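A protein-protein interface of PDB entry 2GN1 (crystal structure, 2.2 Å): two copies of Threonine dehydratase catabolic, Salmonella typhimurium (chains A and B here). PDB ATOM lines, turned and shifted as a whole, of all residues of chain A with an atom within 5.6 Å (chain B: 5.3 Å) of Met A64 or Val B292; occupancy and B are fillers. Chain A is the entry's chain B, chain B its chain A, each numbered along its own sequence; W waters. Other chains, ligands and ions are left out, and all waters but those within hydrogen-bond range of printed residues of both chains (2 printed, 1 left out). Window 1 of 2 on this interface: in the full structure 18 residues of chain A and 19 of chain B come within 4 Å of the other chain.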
ATOM      1  N   THR A  41     -20.645  27.364  -5.605  1.00  0.00           N
ATOM      2  CA  THR A  41     -21.974  27.071  -5.110  1.00  0.00           C
ATOM      3  C   THR A  41     -22.709  28.353  -4.681  1.00  0.00           C
ATOM      4  O   THR A  41     -22.085  29.379  -4.390  1.00  0.00           O
ATOM      5  CB  THR A  41     -21.891  26.127  -3.896  1.00  0.00           C
ATOM      6  OG1 THR A  41     -21.025  26.706  -2.916  1.00  0.00           O
ATOM      7  CG2 THR A  41     -21.334  24.751  -4.306  1.00  0.00           C
ATOM      8  N   PHE A  61     -23.985  26.774  -0.162  1.00  0.00           N
ATOM      9  CA  PHE A  61     -24.515  25.457  -0.547  1.00  0.00           C
ATOM     10  C   PHE A  61     -23.499  24.434  -1.066  1.00  0.00           C
ATOM     11  O   PHE A  61     -23.565  24.043  -2.227  1.00  0.00           O
ATOM     12  CB  PHE A  61     -25.620  25.633  -1.599  1.00  0.00           C
ATOM     13  CG  PHE A  61     -26.820  26.389  -1.105  1.00  0.00           C
ATOM     14  CD1 PHE A  61     -27.355  26.139   0.152  1.00  0.00           C
ATOM     15  CD2 PHE A  61     -27.434  27.331  -1.917  1.00  0.00           C
ATOM     16  CE1 PHE A  61     -28.463  26.832   0.599  1.00  0.00           C
ATOM     17  CE2 PHE A  61     -28.544  28.022  -1.481  1.00  0.00           C
ATOM     18  CZ  PHE A  61     -29.059  27.780  -0.217  1.00  0.00           C
ATOM     19  N   GLU A  62     -22.608  23.954  -0.201  1.00  0.00           N
ATOM     20  CA  GLU A  62     -21.677  22.865  -0.574  1.00  0.00           C
ATOM     21  C   GLU A  62     -22.362  21.497  -0.664  1.00  0.00           C
ATOM     22  O   GLU A  62     -21.793  20.543  -1.199  1.00  0.00           O
ATOM     23  CB  GLU A  62     -20.508  22.783   0.411  1.00  0.00           C
ATOM     24  CG  GLU A  62     -19.616  23.997   0.383  1.00  0.00           C
ATOM     25  CD  GLU A  62     -19.060  24.265  -1.001  1.00  0.00           C
ATOM     26  OE1 GLU A  62     -18.376  23.371  -1.560  1.00  0.00           O
ATOM     27  OE2 GLU A  62     -19.321  25.366  -1.530  1.00  0.00           O
ATOM     28  N   ASN A  63     -23.578  21.410  -0.123  1.00  0.00           N
ATOM     29  CA  ASN A  63     -24.461  20.273  -0.370  1.00  0.00           C
ATOM     30  C   ASN A  63     -24.789  20.108  -1.859  1.00  0.00           C
ATOM     31  O   ASN A  63     -25.072  19.002  -2.321  1.00  0.00           O
ATOM     32  CB  ASN A  63     -25.757  20.399   0.449  1.00  0.00           C
ATOM     33  CG  ASN A  63     -26.522  21.699   0.177  1.00  0.00           C
ATOM     34  OD1 ASN A  63     -25.940  22.710  -0.205  1.00  0.00           O
ATOM     35  ND2 ASN A  63     -27.825  21.676   0.410  1.00  0.00           N
ATOM     36  N   MET A  64     -24.745  21.222  -2.587  1.00  0.00           N
ATOM     37  CA  MET A  64     -25.012  21.262  -4.027  1.00  0.00           C
ATOM     38  C   MET A  64     -23.730  21.211  -4.848  1.00  0.00           C
ATOM     39  O   MET A  64     -23.772  21.348  -6.079  1.00  0.00           O
ATOM     40  CB  MET A  64     -25.792  22.530  -4.374  1.00  0.00           C
ATOM     41  CG  MET A  64     -27.040  22.693  -3.545  1.00  0.00           C
ATOM     42  SD  MET A  64     -28.039  24.117  -4.004  1.00  0.00           S
ATOM     43  CE  MET A  64     -29.126  24.158  -2.576  1.00  0.00           C
ATOM     44  N   GLN A  65     -22.592  21.025  -4.175  1.00  0.00           N
ATOM     45  CA  GLN A  65     -21.330  20.724  -4.851  1.00  0.00           C
ATOM     46  C   GLN A  65     -21.401  19.267  -5.305  1.00  0.00           C
ATOM     47  O   GLN A  65     -22.230  18.501  -4.805  1.00  0.00           O
ATOM     48  CB  GLN A  65     -20.130  20.965  -3.914  1.00  0.00           C
ATOM     49  CG  GLN A  65     -18.747  20.884  -4.580  1.00  0.00           C
ATOM     50  CD  GLN A  65     -18.598  21.822  -5.761  1.00  0.00           C
ATOM     51  OE1 GLN A  65     -18.858  21.443  -6.903  1.00  0.00           O
ATOM     52  NE2 GLN A  65     -18.209  23.054  -5.495  1.00  0.00           N
ATOM     53  N   ARG A  66     -20.557  18.900  -6.268  1.00  0.00           N
ATOM     54  CA  ARG A  66     -20.540  17.548  -6.836  1.00  0.00           C
ATOM     55  C   ARG A  66     -20.342  16.472  -5.776  1.00  0.00           C
ATOM     56  O   ARG A  66     -19.528  16.631  -4.864  1.00  0.00           O
ATOM     57  CB  ARG A  66     -19.454  17.429  -7.914  1.00  0.00           C
ATOM     58  CG  ARG A  66     -19.803  18.176  -9.198  1.00  0.00           C
ATOM     59  CD  ARG A  66     -18.617  18.358 -10.146  1.00  0.00           C
ATOM     60  NE  ARG A  66     -18.213  17.126 -10.827  1.00  0.00           N
ATOM     61  CZ  ARG A  66     -18.913  16.510 -11.782  1.00  0.00           C
ATOM     62  NH1 ARG A  66     -20.090  16.978 -12.184  1.00  0.00           N
ATOM     63  NH2 ARG A  66     -18.441  15.398 -12.332  1.00  0.00           N
ATOM     64  N   GLY A  68     -22.420  15.723  -3.509  1.00  0.00           N
ATOM     65  CA  GLY A  68     -23.334  16.056  -2.415  1.00  0.00           C
ATOM     66  C   GLY A  68     -22.660  16.640  -1.190  1.00  0.00           C
ATOM     67  O   GLY A  68     -23.314  16.903  -0.188  1.00  0.00           O
ATOM     68  N   LYS A 291     -35.812  25.278   2.126  1.00  0.00           N
ATOM     69  CA  LYS A 291     -35.984  24.359   0.998  1.00  0.00           C
ATOM     70  C   LYS A 291     -34.683  23.739   0.496  1.00  0.00           C
ATOM     71  O   LYS A 291     -34.574  23.397  -0.675  1.00  0.00           O
ATOM     72  CB  LYS A 291     -36.713  25.063  -0.157  1.00  0.00           C
ATOM     73  CG  LYS A 291     -37.986  25.781   0.251  1.00  0.00           C
ATOM     74  CD  LYS A 291     -38.999  24.832   0.847  1.00  0.00           C
ATOM     75  CE  LYS A 291     -40.272  25.542   1.253  1.00  0.00           C
ATOM     76  NZ  LYS A 291     -41.293  24.549   1.643  1.00  0.00           N
ATOM     77  N   VAL A 292     -33.699  23.576   1.376  1.00  0.00           N
ATOM     78  CA  VAL A 292     -32.470  22.898   0.977  1.00  0.00           C
ATOM     79  C   VAL A 292     -32.278  21.630   1.784  1.00  0.00           C
ATOM     80  O   VAL A 292     -32.442  21.635   3.005  1.00  0.00           O
ATOM     81  CB  VAL A 292     -31.229  23.810   1.072  1.00  0.00           C
ATOM     82  CG1 VAL A 292     -31.465  25.076   0.281  1.00  0.00           C
ATOM     83  CG2 VAL A 292     -30.879  24.134   2.505  1.00  0.00           C
ATOM     84  N   ILE A 293     -31.941  20.546   1.085  1.00  0.00           N
ATOM     85  CA  ILE A 293     -31.702  19.257   1.723  1.00  0.00           C
ATOM     86  C   ILE A 293     -30.318  19.257   2.360  1.00  0.00           C
ATOM     87  O   ILE A 293     -29.293  19.368   1.668  1.00  0.00           O
ATOM     88  CB  ILE A 293     -31.834  18.081   0.728  1.00  0.00           C
ATOM     89  CG1 ILE A 293     -33.245  18.031   0.115  1.00  0.00           C
ATOM     90  CG2 ILE A 293     -31.496  16.749   1.411  1.00  0.00           C
ATOM     91  CD1 ILE A 293     -34.361  17.722   1.112  1.00  0.00           C
ATOM     92  N   ILE A 323     -23.139  25.095   4.422  1.00  0.00           N
ATOM     93  CA  ILE A 323     -23.904  23.854   4.286  1.00  0.00           C
ATOM     94  C   ILE A 323     -22.981  22.819   3.639  1.00  0.00           C
ATOM     95  O   ILE A 323     -22.946  22.678   2.429  1.00  0.00           O
ATOM     96  CB  ILE A 323     -25.183  24.043   3.417  1.00  0.00           C
ATOM     97  CG1 ILE A 323     -25.972  25.302   3.810  1.00  0.00           C
ATOM     98  CG2 ILE A 323     -26.089  22.805   3.504  1.00  0.00           C
ATOM     99  CD1 ILE A 323     -26.423  25.349   5.265  1.00  0.00           C
ATOM    100  N   PRO B  44     -27.655  30.326  -8.334  1.00  0.00           N
ATOM    101  CA  PRO B  44     -26.403  29.625  -8.609  1.00  0.00           C
ATOM    102  C   PRO B  44     -26.441  28.757  -9.864  1.00  0.00           C
ATOM    103  O   PRO B  44     -27.515  28.328 -10.298  1.00  0.00           O
ATOM    104  CB  PRO B  44     -26.237  28.738  -7.379  1.00  0.00           C
ATOM    105  CG  PRO B  44     -27.648  28.383  -7.023  1.00  0.00           C
ATOM    106  CD  PRO B  44     -28.416  29.663  -7.255  1.00  0.00           C
ATOM    107  N   ASN B  47     -24.763  22.075 -11.121  1.00  0.00           N
ATOM    108  CA  ASN B  47     -23.857  21.047 -11.646  1.00  0.00           C
ATOM    109  C   ASN B  47     -24.573  20.017 -12.479  1.00  0.00           C
ATOM    110  O   ASN B  47     -24.176  19.730 -13.614  1.00  0.00           O
ATOM    111  CB  ASN B  47     -23.124  20.310 -10.516  1.00  0.00           C
ATOM    112  CG  ASN B  47     -22.050  21.148  -9.881  1.00  0.00           C
ATOM    113  OD1 ASN B  47     -21.290  21.816 -10.577  1.00  0.00           O
ATOM    114  ND2 ASN B  47     -21.984  21.127  -8.555  1.00  0.00           N
ATOM    115  N   LEU B  59     -30.145  28.429 -11.485  1.00  0.00           N
ATOM    116  CA  LEU B  59     -31.438  28.170 -10.841  1.00  0.00           C
ATOM    117  C   LEU B  59     -31.851  29.342  -9.966  1.00  0.00           C
ATOM    118  O   LEU B  59     -31.206  29.615  -8.958  1.00  0.00           O
ATOM    119  CB  LEU B  59     -31.364  26.895  -9.994  1.00  0.00           C
ATOM    120  CG  LEU B  59     -30.918  25.598 -10.675  1.00  0.00           C
ATOM    121  CD1 LEU B  59     -30.770  24.502  -9.634  1.00  0.00           C
ATOM    122  CD2 LEU B  59     -31.868  25.159 -11.764  1.00  0.00           C
ATOM    123  N   PHE B  61     -34.005  30.761  -7.236  1.00  0.00           N
ATOM    124  CA  PHE B  61     -34.675  30.101  -6.105  1.00  0.00           C
ATOM    125  C   PHE B  61     -35.849  30.863  -5.470  1.00  0.00           C
ATOM    126  O   PHE B  61     -35.785  31.267  -4.300  1.00  0.00           O
ATOM    127  CB  PHE B  61     -33.643  29.768  -5.014  1.00  0.00           C
ATOM    128  CG  PHE B  61     -32.662  28.688  -5.392  1.00  0.00           C
ATOM    129  CD1 PHE B  61     -33.060  27.560  -6.103  1.00  0.00           C
ATOM    130  CD2 PHE B  61     -31.336  28.783  -4.994  1.00  0.00           C
ATOM    131  CE1 PHE B  61     -32.145  26.565  -6.427  1.00  0.00           C
ATOM    132  CE2 PHE B  61     -30.425  27.801  -5.309  1.00  0.00           C
ATOM    133  CZ  PHE B  61     -30.821  26.691  -6.031  1.00  0.00           C
ATOM    134  N   ASN B  63     -38.447  29.399  -4.682  1.00  0.00           N
ATOM    135  CA  ASN B  63     -38.830  28.458  -3.639  1.00  0.00           C
ATOM    136  C   ASN B  63     -38.311  28.880  -2.254  1.00  0.00           C
ATOM    137  O   ASN B  63     -38.892  28.516  -1.236  1.00  0.00           O
ATOM    138  CB  ASN B  63     -38.376  27.032  -4.000  1.00  0.00           C
ATOM    139  CG  ASN B  63     -36.848  26.889  -4.141  1.00  0.00           C
ATOM    140  OD1 ASN B  63     -36.150  27.800  -4.586  1.00  0.00           O
ATOM    141  ND2 ASN B  63     -36.339  25.713  -3.775  1.00  0.00           N
ATOM    142  N   MET B  64     -37.231  29.660  -2.235  1.00  0.00           N
ATOM    143  CA  MET B  64     -36.676  30.229  -1.005  1.00  0.00           C
ATOM    144  C   MET B  64     -37.116  31.679  -0.749  1.00  0.00           C
ATOM    145  O   MET B  64     -36.638  32.324   0.198  1.00  0.00           O
ATOM    146  CB  MET B  64     -35.155  30.163  -1.046  1.00  0.00           C
ATOM    147  CG  MET B  64     -34.633  28.793  -1.368  1.00  0.00           C
ATOM    148  SD  MET B  64     -32.845  28.706  -1.445  1.00  0.00           S
ATOM    149  CE  MET B  64     -32.672  27.018  -2.044  1.00  0.00           C
ATOM    150  N   LEU B 286     -33.914  17.829  -9.094  1.00  0.00           N
ATOM    151  CA  LEU B 286     -33.727  18.995  -8.240  1.00  0.00           C
ATOM    152  C   LEU B 286     -33.486  18.602  -6.781  1.00  0.00           C
ATOM    153  O   LEU B 286     -32.602  19.162  -6.127  1.00  0.00           O
ATOM    154  CB  LEU B 286     -34.902  19.972  -8.374  1.00  0.00           C
ATOM    155  CG  LEU B 286     -34.872  20.782  -9.674  1.00  0.00           C
ATOM    156  CD1 LEU B 286     -36.225  21.426  -9.958  1.00  0.00           C
ATOM    157  CD2 LEU B 286     -33.763  21.834  -9.648  1.00  0.00           C
ATOM    158  N   ILE B 287     -34.224  17.610  -6.286  1.00  0.00           N
ATOM    159  CA  ILE B 287     -34.087  17.205  -4.882  1.00  0.00           C
ATOM    160  C   ILE B 287     -32.883  16.291  -4.649  1.00  0.00           C
ATOM    161  O   ILE B 287     -32.089  16.542  -3.743  1.00  0.00           O
ATOM    162  CB  ILE B 287     -35.398  16.572  -4.333  1.00  0.00           C
ATOM    163  CG1 ILE B 287     -36.588  17.522  -4.562  1.00  0.00           C
ATOM    164  CG2 ILE B 287     -35.264  16.285  -2.833  1.00  0.00           C
ATOM    165  CD1 ILE B 287     -37.924  16.819  -4.797  1.00  0.00           C
ATOM    166  N   ASN B 290     -29.619  18.118  -6.822  1.00  0.00           N
ATOM    167  CA  ASN B 290     -29.357  19.518  -6.490  1.00  0.00           C
ATOM    168  C   ASN B 290     -29.757  19.945  -5.074  1.00  0.00           C
ATOM    169  O   ASN B 290     -29.578  21.104  -4.712  1.00  0.00           O
ATOM    170  CB  ASN B 290     -30.019  20.430  -7.523  1.00  0.00           C
ATOM    171  CG  ASN B 290     -29.114  21.565  -7.950  1.00  0.00           C
ATOM    172  OD1 ASN B 290     -28.816  21.721  -9.134  1.00  0.00           O
ATOM    173  ND2 ASN B 290     -28.655  22.351  -6.986  1.00  0.00           N
ATOM    174  N   LYS B 291     -30.295  19.012  -4.288  1.00  0.00           N
ATOM    175  CA  LYS B 291     -30.584  19.220  -2.863  1.00  0.00           C
ATOM    176  C   LYS B 291     -31.499  20.407  -2.575  1.00  0.00           C
ATOM    177  O   LYS B 291     -31.382  21.058  -1.541  1.00  0.00           O
ATOM    178  CB  LYS B 291     -29.277  19.328  -2.065  1.00  0.00           C
ATOM    179  CG  LYS B 291     -28.320  18.173  -2.288  1.00  0.00           C
ATOM    180  CD  LYS B 291     -28.934  16.822  -1.907  1.00  0.00           C
ATOM    181  CE  LYS B 291     -28.009  15.661  -2.208  1.00  0.00           C
ATOM    182  NZ  LYS B 291     -28.517  14.374  -1.625  1.00  0.00           N
ATOM    183  N   VAL B 292     -32.433  20.672  -3.484  1.00  0.00           N
ATOM    184  CA  VAL B 292     -33.418  21.724  -3.263  1.00  0.00           C
ATOM    185  C   VAL B 292     -34.831  21.157  -3.334  1.00  0.00           C
ATOM    186  O   VAL B 292     -35.129  20.308  -4.183  1.00  0.00           O
ATOM    187  CB  VAL B 292     -33.257  22.907  -4.255  1.00  0.00           C
ATOM    188  CG1 VAL B 292     -32.104  23.811  -3.824  1.00  0.00           C
ATOM    189  CG2 VAL B 292     -33.026  22.414  -5.680  1.00  0.00           C
ATOM    190  N   ILE B 293     -35.681  21.612  -2.417  1.00  0.00           N
ATOM    191  CA  ILE B 293     -37.088  21.219  -2.402  1.00  0.00           C
ATOM    192  C   ILE B 293     -37.877  22.136  -3.339  1.00  0.00           C
ATOM    193  O   ILE B 293     -37.855  23.370  -3.212  1.00  0.00           O
ATOM    194  CB  ILE B 293     -37.684  21.250  -0.985  1.00  0.00           C
ATOM    195  CG1 ILE B 293     -36.948  20.240  -0.101  1.00  0.00           C
ATOM    196  CG2 ILE B 293     -39.177  20.922  -1.004  1.00  0.00           C
ATOM    197  CD1 ILE B 293     -37.296  20.347   1.351  1.00  0.00           C
ATOM    198  N   THR B 294     -38.565  21.503  -4.280  1.00  0.00           N
ATOM    199  CA  THR B 294     -39.390  22.187  -5.257  1.00  0.00           C
ATOM    200  C   THR B 294     -40.731  21.481  -5.308  1.00  0.00           C
ATOM    201  O   THR B 294     -40.804  20.259  -5.166  1.00  0.00           O
ATOM    202  CB  THR B 294     -38.738  22.172  -6.680  1.00  0.00           C
ATOM    203  OG1 THR B 294     -39.637  22.757  -7.635  1.00  0.00           O
ATOM    204  CG2 THR B 294     -38.402  20.758  -7.125  1.00  0.00           C
HETATM  205  O   HOH W   1     -25.492  22.034  -8.235  1.00  0.00           O
HETATM  206  O   HOH W   2     -24.182  18.682  -7.561  1.00  0.00           O
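Among the printed residues, merely in contact across the chains: Asn A63 with Lys B291 (3.4 Å), Met A64 with Lys B291 (3.97 Å), Met A64 with Val B292 (3.2 Å), Gln A65 with Asn B47 (3.5 Å), Lys A291 with Asn B63 (3.2 Å), Lys A291 with Val B292 (3.3 Å), Val A292 with Met B64 (3.3 Å), Val A292 with Lys B291 (3.3 Å), Ile A293 with Ile B287 (3.98 Å) and Ile A293 with Ile B293 (3.8 Å).
Met A64 touches Val B292, and with the chains exchanged Val A292 touches Met B64.
Lys A291 touches Val B292, and with the chains exchanged Val A292 touches Lys B291.
Lys A291 touches Ile B293, and with the chains exchanged Ile A293 touches Lys B291.
Ile A293 touches its own counterpart, Ile B293.
Of the 15 pairs that touch across the chains among the printed residues, 9 have their exchanged pair printed and touching as well.
O of Phe B61 sits close to OD1 of Asn B63, 3.5 Å away.
ND2 of Asn B63 is in hydrogen-bond range of O of Ile B293 (2.8 Å).
The backbone NH (N) of Lys B291 lies within hydrogen-bond range of the backbone carbonyl oxygen (O) of Leu B286, at 3.0 Å.
The backbone NH (N) of Val B292 lies within hydrogen-bond range of the backbone carbonyl oxygen (O) of Leu B286.
O of Phe A61 lies close to OD1 of Asn A63, 3.4 Å away.
ND2 of Asn A63 is in hydrogen-bond range of O of Ile A293 (3.0 Å).
Water W1 lies within hydrogen-bond range of the backbone carbonyl oxygen (O) of Met A64 (2.8 Å), the backbone NH (N) of Asn B47 (3.0 Å) and the side-chain amide nitrogen (ND2) of Asn B290 (3.4 Å).
Water W2 lies within hydrogen-bond range of O of Met A64 (3.1 Å), O of Gln A65 (3.4 Å) and ND2 of Asn B47 (3.4 Å).
Thr A41 touches none of the printed residues of chain B.
Printed residues of chain B within 4 Å of Asn A63: Lys B291 (3.4 Å).
Of chain B, only Asn B47 (3.1 Å), Asn B290 (3.2 Å), Lys B291 (3.97 Å) and Val B292 (3.2 Å) come within 4 Å of Met A64.
Of the printed residues of chain B, Lys A291 touches Asn B63, Val B292 and Ile B293.
Printed residues of chain B within 4 Å of Val A292: Met B64 (3.3 Å) and Lys B291 (3.3 Å).
Printed residues of chain B within 4 Å of Ile A293: Ile B287, Lys B291 and Ile B293.
Pro B44 touches none of the printed residues of chain A.
Val B292 touches two residues of chain A.
Printed residues of chain A within 4 Å of Ile B293: Lys A291 (2.7 Å) and Ile A293 (3.8 Å).
The nearest residue of chain B that does not touch Met A64 is Phe B61 (4.3 Å).
The nearest printed residue of chain A that does not touch Ile B287 is Lys A291 (7.3 Å).
The side-chain amide nitrogen (ND2) of Asn B47 lies within hydrogen-bond range of the backbone carbonyl oxygen (O) of Met A64 (3.1 Å).
The backbone NH (N) of Arg A66 sits close to the side-chain amide nitrogen (ND2) of Asn B47, at 3.5 Å.
The side-chain sulfur of Met A64 sits at hydrogen-bond distance from the side-chain amide nitrogen of Asn B290 (3.5 Å).
The backbone NH of Ile A293 is in hydrogen-bond range of the backbone carbonyl oxygen of Lys B291 (2.7 Å).
O of Lys A291 is in hydrogen-bond range of N of Ile B293 (2.7 Å).
Of the 13 printed residues of chain B, 8 touch a printed residue of chain A.
Hydrophobic or aromatic side chains of chain B that line the printed part of chain A: Met B64, Ile B287, Val B292 and Ile B293.
Printed residues of chain A that touch a printed residue of chain B: Asn A63, Met A64, Gln A65, Arg A66, Lys A291, Val A292 and Ile A293.
Among the printed residues, 15 pairs touch across the chains.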
